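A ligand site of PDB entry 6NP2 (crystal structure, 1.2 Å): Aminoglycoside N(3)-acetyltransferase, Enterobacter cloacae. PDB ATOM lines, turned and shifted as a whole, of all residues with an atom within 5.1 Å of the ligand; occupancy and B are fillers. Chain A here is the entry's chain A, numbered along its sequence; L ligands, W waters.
A nitrogen (N1) of the ligand sits at hydrogen-bond distance from the side-chain hydroxyl (OH) of Tyr 141, 3.0 Å away.
N1 of the ligand is in hydrogen-bond range of OG of Ser 207, at 2.8 Å.
N3 of the ligand is in hydrogen-bond range of NE2 of His 171 (2.9 Å).
The side-chain amide oxygen (OD1) of Asn 208 sits at hydrogen-bond distance from an oxygen (O5) of the ligand, at 2.7 Å.
OD1 of Asp 118 is in salt-bridge range of N4 of the ligand, at 2.8 Å.
The side-chain carboxylate (OD2) of Asp 165 lies within salt-bridge range of a nitrogen (N2) of the ligand (2.9 Å).
The backbone carbonyl oxygen (O) of Asp 118 sits at hydrogen-bond distance from the side-chain hydroxyl (OG) of Ser 61, at 2.7 Å.
The side-chain carboxylate (OD1) of Asp 118 lies within hydrogen-bond range of the side-chain hydroxyl (OG) of Ser 65, 2.7 Å away.
Ser 61 touches the ligand (OG to C19, 3.2 Å).
Tyr 67 touches the ligand.
OE2 of Glu 68 touches O3 of the ligand, at 3.5 Å.
Tyr 95 touches the ligand.
Phe 98 touches the ligand.
Pro 217 touches the ligand (O to C16, 3.6 Å).
Hydrophobic or aromatic side chains that line the ligand: Tyr 67, Tyr 95, Phe 98, Tyr 141 and His 171.
Of the 20 residues printed, 12 come within 4 Å of the ligand.
Water W1 lies within hydrogen-bond range of N4 of the ligand (2.8 Å) and O of Ser 65 (2.9 Å).
Water W4 lies within hydrogen-bond range of the backbone carbonyl oxygen of Pro 217 (2.8 Å), a nitrogen (N5) of the ligand (2.9 Å) and the side-chain amide oxygen of Asn 208 (3.3 Å).
Water W2 lies within hydrogen-bond range of O of Asp 165 (2.7 Å) and N2 of the ligand (2.9 Å).
Water W6 lies within hydrogen-bond range of the side-chain carboxylate (OD2) of Asp 221, the backbone carbonyl oxygen (O) of Ser 207 and a nitrogen (N5) of the ligand.
Water W9 lies within hydrogen-bond range of O of Ala 216 (2.7 Å), N5 of the ligand (3.0 Å) and O of Asn 208 (3.4 Å).
Water W7 bridges OD1 of Asn 208 (3.2 Å) and O5 of the ligand (3.3 Å).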
ATOM      1  N   PHE A  59     -31.924  -4.309  -7.392  1.00  0.00           N
ATOM      2  CA  PHE A  59     -30.708  -4.263  -8.204  1.00  0.00           C
ATOM      3  C   PHE A  59     -31.012  -4.984  -9.517  1.00  0.00           C
ATOM      4  O   PHE A  59     -31.049  -6.217  -9.557  1.00  0.00           O
ATOM      5  CB  PHE A  59     -29.567  -4.941  -7.452  1.00  0.00           C
ATOM      6  CG  PHE A  59     -28.331  -5.160  -8.287  1.00  0.00           C
ATOM      7  CD1 PHE A  59     -27.879  -4.212  -9.179  1.00  0.00           C
ATOM      8  CD2 PHE A  59     -27.631  -6.341  -8.167  1.00  0.00           C
ATOM      9  CE1 PHE A  59     -26.755  -4.446  -9.932  1.00  0.00           C
ATOM     10  CE2 PHE A  59     -26.502  -6.566  -8.917  1.00  0.00           C
ATOM     11  CZ  PHE A  59     -26.055  -5.619  -9.796  1.00  0.00           C
ATOM     12  N   SER A  61     -29.629  -4.001 -12.841  1.00  0.00           N
ATOM     13  CA  SER A  61     -28.522  -4.007 -13.810  1.00  0.00           C
ATOM     14  C   SER A  61     -29.073  -3.869 -15.233  1.00  0.00           C
ATOM     15  O   SER A  61     -30.093  -3.182 -15.438  1.00  0.00           O
ATOM     16  CB  SER A  61     -27.648  -5.215 -13.569  1.00  0.00           C
ATOM     17  OG  SER A  61     -26.478  -5.214 -14.379  1.00  0.00           O
ATOM     18  N   TRP A  62     -28.407  -4.491 -16.198  1.00  0.00           N
ATOM     19  CA  TRP A  62     -28.713  -4.295 -17.605  1.00  0.00           C
ATOM     20  C   TRP A  62     -28.285  -5.545 -18.354  1.00  0.00           C
ATOM     21  O   TRP A  62     -27.139  -5.971 -18.262  1.00  0.00           O
ATOM     22  CB  TRP A  62     -27.915  -3.100 -18.115  1.00  0.00           C
ATOM     23  CG  TRP A  62     -28.050  -2.779 -19.567  1.00  0.00           C
ATOM     24  CD1 TRP A  62     -29.069  -3.122 -20.414  1.00  0.00           C
ATOM     25  CD2 TRP A  62     -27.135  -1.996 -20.340  1.00  0.00           C
ATOM     26  NE1 TRP A  62     -28.829  -2.609 -21.682  1.00  0.00           N
ATOM     27  CE2 TRP A  62     -27.654  -1.915 -21.650  1.00  0.00           C
ATOM     28  CE3 TRP A  62     -25.930  -1.362 -20.058  1.00  0.00           C
ATOM     29  CZ2 TRP A  62     -27.005  -1.216 -22.665  1.00  0.00           C
ATOM     30  CZ3 TRP A  62     -25.293  -0.671 -21.062  1.00  0.00           C
ATOM     31  CH2 TRP A  62     -25.823  -0.615 -22.348  1.00  0.00           C
ATOM     32  N   SER A  65     -25.112  -4.952 -20.473  1.00  0.00           N
ATOM     33  CA  SER A  65     -23.975  -4.215 -19.947  1.00  0.00           C
ATOM     34  C   SER A  65     -22.671  -4.747 -20.554  1.00  0.00           C
ATOM     35  O   SER A  65     -22.408  -5.953 -20.471  1.00  0.00           O
ATOM     36  CB  SER A  65     -23.922  -4.423 -18.450  1.00  0.00           C
ATOM     37  OG  SER A  65     -22.730  -3.856 -17.967  1.00  0.00           O
ATOM     38  N   TYR A  67     -19.760  -5.087 -19.508  1.00  0.00           N
ATOM     39  CA  TYR A  67     -18.806  -5.221 -18.418  1.00  0.00           C
ATOM     40  C   TYR A  67     -17.617  -6.086 -18.824  1.00  0.00           C
ATOM     41  O   TYR A  67     -16.461  -5.635 -18.839  1.00  0.00           O
ATOM     42  CB  TYR A  67     -19.520  -5.816 -17.205  1.00  0.00           C
ATOM     43  CG  TYR A  67     -18.696  -5.871 -15.946  1.00  0.00           C
ATOM     44  CD1 TYR A  67     -18.698  -4.819 -15.049  1.00  0.00           C
ATOM     45  CD2 TYR A  67     -17.933  -7.004 -15.635  1.00  0.00           C
ATOM     46  CE1 TYR A  67     -17.952  -4.854 -13.885  1.00  0.00           C
ATOM     47  CE2 TYR A  67     -17.184  -7.043 -14.462  1.00  0.00           C
ATOM     48  CZ  TYR A  67     -17.214  -5.967 -13.592  1.00  0.00           C
ATOM     49  OH  TYR A  67     -16.486  -5.965 -12.427  1.00  0.00           O
ATOM     50  N   GLU A  68     -17.866  -7.350 -19.188  1.00  0.00           N
ATOM     51  CA  GLU A  68     -16.759  -8.234 -19.522  1.00  0.00           C
ATOM     52  C   GLU A  68     -16.024  -7.732 -20.753  1.00  0.00           C
ATOM     53  O   GLU A  68     -14.805  -7.907 -20.868  1.00  0.00           O
ATOM     54  CB  GLU A  68     -17.275  -9.655 -19.738  1.00  0.00           C
ATOM     55  CG  GLU A  68     -17.965 -10.254 -18.522  1.00  0.00           C
ATOM     56  CD  GLU A  68     -17.051 -10.376 -17.311  1.00  0.00           C
ATOM     57  OE1 GLU A  68     -15.812 -10.324 -17.480  1.00  0.00           O
ATOM     58  OE2 GLU A  68     -17.571 -10.506 -16.175  1.00  0.00           O
ATOM     59  N   TYR A  95     -30.832  -7.374 -16.179  1.00  0.00           N
ATOM     60  CA  TYR A  95     -29.919  -8.508 -16.374  1.00  0.00           C
ATOM     61  C   TYR A  95     -30.572  -9.791 -15.881  1.00  0.00           C
ATOM     62  O   TYR A  95     -30.882  -9.902 -14.692  1.00  0.00           O
ATOM     63  CB  TYR A  95     -28.609  -8.275 -15.619  1.00  0.00           C
ATOM     64  CG  TYR A  95     -27.588  -9.357 -15.889  1.00  0.00           C
ATOM     65  CD1 TYR A  95     -26.956  -9.431 -17.113  1.00  0.00           C
ATOM     66  CD2 TYR A  95     -27.282 -10.311 -14.930  1.00  0.00           C
ATOM     67  CE1 TYR A  95     -26.037 -10.424 -17.377  1.00  0.00           C
ATOM     68  CE2 TYR A  95     -26.358 -11.312 -15.177  1.00  0.00           C
ATOM     69  CZ  TYR A  95     -25.747 -11.371 -16.410  1.00  0.00           C
ATOM     70  OH  TYR A  95     -24.826 -12.351 -16.681  1.00  0.00           O
ATOM     71  N   PHE A  98     -29.752 -11.855 -12.289  1.00  0.00           N
ATOM     72  CA  PHE A  98     -30.046 -11.399 -10.936  1.00  0.00           C
ATOM     73  C   PHE A  98     -31.489 -11.666 -10.562  1.00  0.00           C
ATOM     74  O   PHE A  98     -31.900 -11.317  -9.449  1.00  0.00           O
ATOM     75  CB  PHE A  98     -29.673  -9.927 -10.781  1.00  0.00           C
ATOM     76  CG  PHE A  98     -28.223  -9.641 -11.114  1.00  0.00           C
ATOM     77  CD1 PHE A  98     -27.222 -10.587 -10.871  1.00  0.00           C
ATOM     78  CD2 PHE A  98     -27.849  -8.450 -11.677  1.00  0.00           C
ATOM     79  CE1 PHE A  98     -25.904 -10.306 -11.191  1.00  0.00           C
ATOM     80  CE2 PHE A  98     -26.536  -8.194 -11.985  1.00  0.00           C
ATOM     81  CZ  PHE A  98     -25.573  -9.116 -11.742  1.00  0.00           C
ATOM     82  N   ASP A 118     -24.308  -0.582 -15.286  1.00  0.00           N
ATOM     83  CA  ASP A 118     -24.017  -1.923 -14.793  1.00  0.00           C
ATOM     84  C   ASP A 118     -24.624  -2.179 -13.430  1.00  0.00           C
ATOM     85  O   ASP A 118     -25.056  -3.297 -13.137  1.00  0.00           O
ATOM     86  CB  ASP A 118     -22.503  -2.186 -14.761  1.00  0.00           C
ATOM     87  CG  ASP A 118     -22.191  -3.651 -14.509  1.00  0.00           C
ATOM     88  OD1 ASP A 118     -22.485  -4.487 -15.397  1.00  0.00           O
ATOM     89  OD2 ASP A 118     -21.679  -3.942 -13.417  1.00  0.00           O
ATOM     90  N   TYR A 141     -21.917   0.559  -5.555  1.00  0.00           N
ATOM     91  CA  TYR A 141     -22.630   0.032  -4.401  1.00  0.00           C
ATOM     92  C   TYR A 141     -22.240   0.697  -3.084  1.00  0.00           C
ATOM     93  O   TYR A 141     -22.738   0.295  -2.033  1.00  0.00           O
ATOM     94  CB  TYR A 141     -22.432  -1.495  -4.263  1.00  0.00           C
ATOM     95  CG  TYR A 141     -22.681  -2.197  -5.559  1.00  0.00           C
ATOM     96  CD1 TYR A 141     -23.954  -2.338  -6.093  1.00  0.00           C
ATOM     97  CD2 TYR A 141     -21.620  -2.676  -6.300  1.00  0.00           C
ATOM     98  CE1 TYR A 141     -24.151  -2.935  -7.317  1.00  0.00           C
ATOM     99  CE2 TYR A 141     -21.822  -3.282  -7.526  1.00  0.00           C
ATOM    100  CZ  TYR A 141     -23.096  -3.407  -8.030  1.00  0.00           C
ATOM    101  OH  TYR A 141     -23.312  -3.976  -9.268  1.00  0.00           O
ATOM    102  N   ASP A 165     -25.240 -15.550  -1.142  1.00  0.00           N
ATOM    103  CA  ASP A 165     -24.452 -14.758  -2.070  1.00  0.00           C
ATOM    104  C   ASP A 165     -25.229 -13.608  -2.680  1.00  0.00           C
ATOM    105  O   ASP A 165     -24.623 -12.710  -3.260  1.00  0.00           O
ATOM    106  CB  ASP A 165     -23.976 -15.641  -3.226  1.00  0.00           C
ATOM    107  CG  ASP A 165     -25.140 -16.156  -4.049  1.00  0.00           C
ATOM    108  OD1 ASP A 165     -25.943 -16.940  -3.506  1.00  0.00           O
ATOM    109  OD2 ASP A 165     -25.305 -15.735  -5.211  1.00  0.00           O
ATOM    110  N   HIS A 171     -22.128  -5.318  -0.674  1.00  0.00           N
ATOM    111  CA  HIS A 171     -21.051  -4.654  -1.403  1.00  0.00           C
ATOM    112  C   HIS A 171     -20.758  -3.264  -0.861  1.00  0.00           C
ATOM    113  O   HIS A 171     -19.649  -2.762  -1.057  1.00  0.00           O
ATOM    114  CB  HIS A 171     -21.354  -4.619  -2.892  1.00  0.00           C
ATOM    115  CG  HIS A 171     -21.409  -5.972  -3.530  1.00  0.00           C
ATOM    116  ND1 HIS A 171     -20.326  -6.833  -3.533  1.00  0.00           N
ATOM    117  CD2 HIS A 171     -22.389  -6.606  -4.199  1.00  0.00           C
ATOM    118  CE1 HIS A 171     -20.661  -7.952  -4.146  1.00  0.00           C
ATOM    119  NE2 HIS A 171     -21.911  -7.835  -4.570  1.00  0.00           N
ATOM    120  N   SER A 207     -16.715  -6.042  -7.584  1.00  0.00           N
ATOM    121  CA  SER A 207     -17.904  -6.649  -7.003  1.00  0.00           C
ATOM    122  C   SER A 207     -17.929  -8.150  -7.192  1.00  0.00           C
ATOM    123  O   SER A 207     -18.887  -8.797  -6.766  1.00  0.00           O
ATOM    124  CB  SER A 207     -19.179  -6.020  -7.591  1.00  0.00           C
ATOM    125  OG  SER A 207     -19.353  -6.369  -8.950  1.00  0.00           O
ATOM    126  N   ASN A 208     -16.892  -8.732  -7.794  1.00  0.00           N
ATOM    127  CA  ASN A 208     -16.742 -10.178  -7.890  1.00  0.00           C
ATOM    128  C   ASN A 208     -15.657 -10.703  -6.965  1.00  0.00           C
ATOM    129  O   ASN A 208     -15.128 -11.797  -7.202  1.00  0.00           O
ATOM    130  CB  ASN A 208     -16.491 -10.604  -9.330  1.00  0.00           C
ATOM    131  CG  ASN A 208     -17.754 -10.524 -10.162  1.00  0.00           C
ATOM    132  OD1 ASN A 208     -18.770 -11.103  -9.789  1.00  0.00           O
ATOM    133  ND2 ASN A 208     -17.708  -9.792 -11.252  1.00  0.00           N
ATOM    134  N   GLY A 209     -15.306  -9.961  -5.932  1.00  0.00           N
ATOM    135  CA  GLY A 209     -14.367 -10.415  -4.929  1.00  0.00           C
ATOM    136  C   GLY A 209     -13.508  -9.261  -4.450  1.00  0.00           C
ATOM    137  O   GLY A 209     -12.675  -8.761  -5.213  1.00  0.00           O
ATOM    138  N   ALA A 216     -12.507 -16.118  -6.378  1.00  0.00           N
ATOM    139  CA  ALA A 216     -12.692 -17.277  -7.251  1.00  0.00           C
ATOM    140  C   ALA A 216     -13.948 -17.099  -8.092  1.00  0.00           C
ATOM    141  O   ALA A 216     -14.972 -16.620  -7.581  1.00  0.00           O
ATOM    142  CB  ALA A 216     -12.801 -18.553  -6.414  1.00  0.00           C
ATOM    143  N   PRO A 217     -13.929 -17.468  -9.391  1.00  0.00           N
ATOM    144  CA  PRO A 217     -15.105 -17.248 -10.258  1.00  0.00           C
ATOM    145  C   PRO A 217     -16.424 -17.725  -9.667  1.00  0.00           C
ATOM    146  O   PRO A 217     -17.388 -16.951  -9.591  1.00  0.00           O
ATOM    147  CB  PRO A 217     -14.744 -18.029 -11.538  1.00  0.00           C
ATOM    148  CG  PRO A 217     -13.268 -17.930 -11.603  1.00  0.00           C
ATOM    149  CD  PRO A 217     -12.762 -17.942 -10.172  1.00  0.00           C
ATOM    150  N   ASP A 218     -16.489 -18.991  -9.265  1.00  0.00           N
ATOM    151  CA  ASP A 218     -17.591 -19.494  -8.449  1.00  0.00           C
ATOM    152  C   ASP A 218     -17.075 -19.490  -7.013  1.00  0.00           C
ATOM    153  O   ASP A 218     -16.278 -20.347  -6.632  1.00  0.00           O
ATOM    154  CB  ASP A 218     -18.062 -20.881  -8.868  1.00  0.00           C
ATOM    155  CG  ASP A 218     -16.946 -21.758  -9.397  1.00  0.00           C
ATOM    156  OD1 ASP A 218     -16.273 -21.358 -10.373  1.00  0.00           O
ATOM    157  OD2 ASP A 218     -16.742 -22.864  -8.843  1.00  0.00           O
ATOM    158  N   GLY A 219     -17.543 -18.506  -6.236  1.00  0.00           N
ATOM    159  CA  GLY A 219     -16.931 -18.100  -4.985  1.00  0.00           C
ATOM    160  C   GLY A 219     -16.517 -19.217  -4.047  1.00  0.00           C
ATOM    161  O   GLY A 219     -15.863 -20.182  -4.441  1.00  0.00           O
ATOM    162  N   ASP A 221     -17.614 -15.616  -2.380  1.00  0.00           N
ATOM    163  CA  ASP A 221     -17.078 -14.288  -2.182  1.00  0.00           C
ATOM    164  C   ASP A 221     -17.308 -13.854  -0.733  1.00  0.00           C
ATOM    165  O   ASP A 221     -17.821 -14.609   0.100  1.00  0.00           O
ATOM    166  CB  ASP A 221     -17.661 -13.309  -3.198  1.00  0.00           C
ATOM    167  CG  ASP A 221     -19.125 -12.960  -2.937  1.00  0.00           C
ATOM    168  OD1 ASP A 221     -19.802 -13.679  -2.190  1.00  0.00           O
ATOM    169  OD2 ASP A 221     -19.560 -11.956  -3.510  1.00  0.00           O
HETATM  170  C1  LIG L   1     -21.996 -13.228  -8.606  1.00  0.00           C
HETATM  171  C2  LIG L   1     -22.452  -8.049  -9.371  1.00  0.00           C
HETATM  172  C3  LIG L   1     -20.833  -8.222 -12.360  1.00  0.00           C
HETATM  173  C4  LIG L   1     -22.980 -14.391  -8.523  1.00  0.00           C
HETATM  174  C5  LIG L   1     -22.230  -8.350  -7.888  1.00  0.00           C
HETATM  175  C6  LIG L   1     -21.463  -7.323 -13.415  1.00  0.00           C
HETATM  176  C7  LIG L   1     -22.230 -15.670  -8.940  1.00  0.00           C
HETATM  177  C8  LIG L   1     -22.738  -9.757  -7.614  1.00  0.00           C
HETATM  178  C9  LIG L   1     -22.361  -8.154 -14.334  1.00  0.00           C
HETATM  179  C10 LIG L   1     -20.870 -15.715  -8.304  1.00  0.00           C
HETATM  180  C11 LIG L   1     -22.038 -10.785  -8.492  1.00  0.00           C
HETATM  181  C12 LIG L   1     -21.568  -9.316 -14.936  1.00  0.00           C
HETATM  182  C13 LIG L   1     -20.323 -14.672  -7.732  1.00  0.00           C
HETATM  183  C14 LIG L   1     -22.151 -10.448  -9.965  1.00  0.00           C
HETATM  184  C15 LIG L   1     -20.865 -10.118 -13.831  1.00  0.00           C
HETATM  185  C16 LIG L   1     -18.935 -14.806  -7.148  1.00  0.00           C
HETATM  186  C17 LIG L   1     -21.664  -9.033 -10.217  1.00  0.00           C
HETATM  187  C18 LIG L   1     -22.507 -10.291 -15.661  1.00  0.00           C
HETATM  188  C19 LIG L   1     -24.377  -7.339 -15.516  1.00  0.00           C
HETATM  189  N1  LIG L   1     -22.033  -6.674  -9.670  1.00  0.00           N
HETATM  190  N2  LIG L   1     -23.500 -14.496  -7.155  1.00  0.00           N
HETATM  191  N3  LIG L   1     -22.525 -10.137  -6.215  1.00  0.00           N
HETATM  192  N4  LIG L   1     -22.896  -7.282 -15.418  1.00  0.00           N
HETATM  193  N5  LIG L   1     -18.181 -13.570  -7.382  1.00  0.00           N
HETATM  194  O1  LIG L   1     -22.686 -12.038  -8.227  1.00  0.00           O
HETATM  195  O2  LIG L   1     -22.286  -6.378 -12.763  1.00  0.00           O
HETATM  196  O3  LIG L   1     -20.614  -8.754 -15.830  1.00  0.00           O
HETATM  197  O4  LIG L   1     -20.928 -13.467  -7.694  1.00  0.00           O
HETATM  198  O5  LIG L   1     -21.333 -11.345 -10.718  1.00  0.00           O
HETATM  199  O6  LIG L   1     -20.099  -9.270 -12.969  1.00  0.00           O
HETATM  200  O7  LIG L   1     -21.899  -8.768 -11.599  1.00  0.00           O
HETATM  201  O   HOH W   1     -22.626  -7.790 -18.209  1.00  0.00           O
HETATM  202  O   HOH W   2     -24.663 -12.126  -5.866  1.00  0.00           O
HETATM  203  O   HOH W   3     -25.828  -9.056  -5.981  1.00  0.00           O
HETATM  204  O   HOH W   4     -17.556 -14.197 -10.093  1.00  0.00           O
HETATM  205  O   HOH W   5     -22.159 -13.496 -12.249  1.00  0.00           O
HETATM  206  O   HOH W   6     -19.565 -11.326  -6.023  1.00  0.00           O
HETATM  207  O   HOH W   7     -19.084 -13.388 -11.950  1.00  0.00           O
HETATM  208  O   HOH W   8     -22.173 -12.290  -4.240  1.00  0.00           O
HETATM  209  O   HOH W   9     -15.954 -14.839  -5.853  1.00  0.00           O
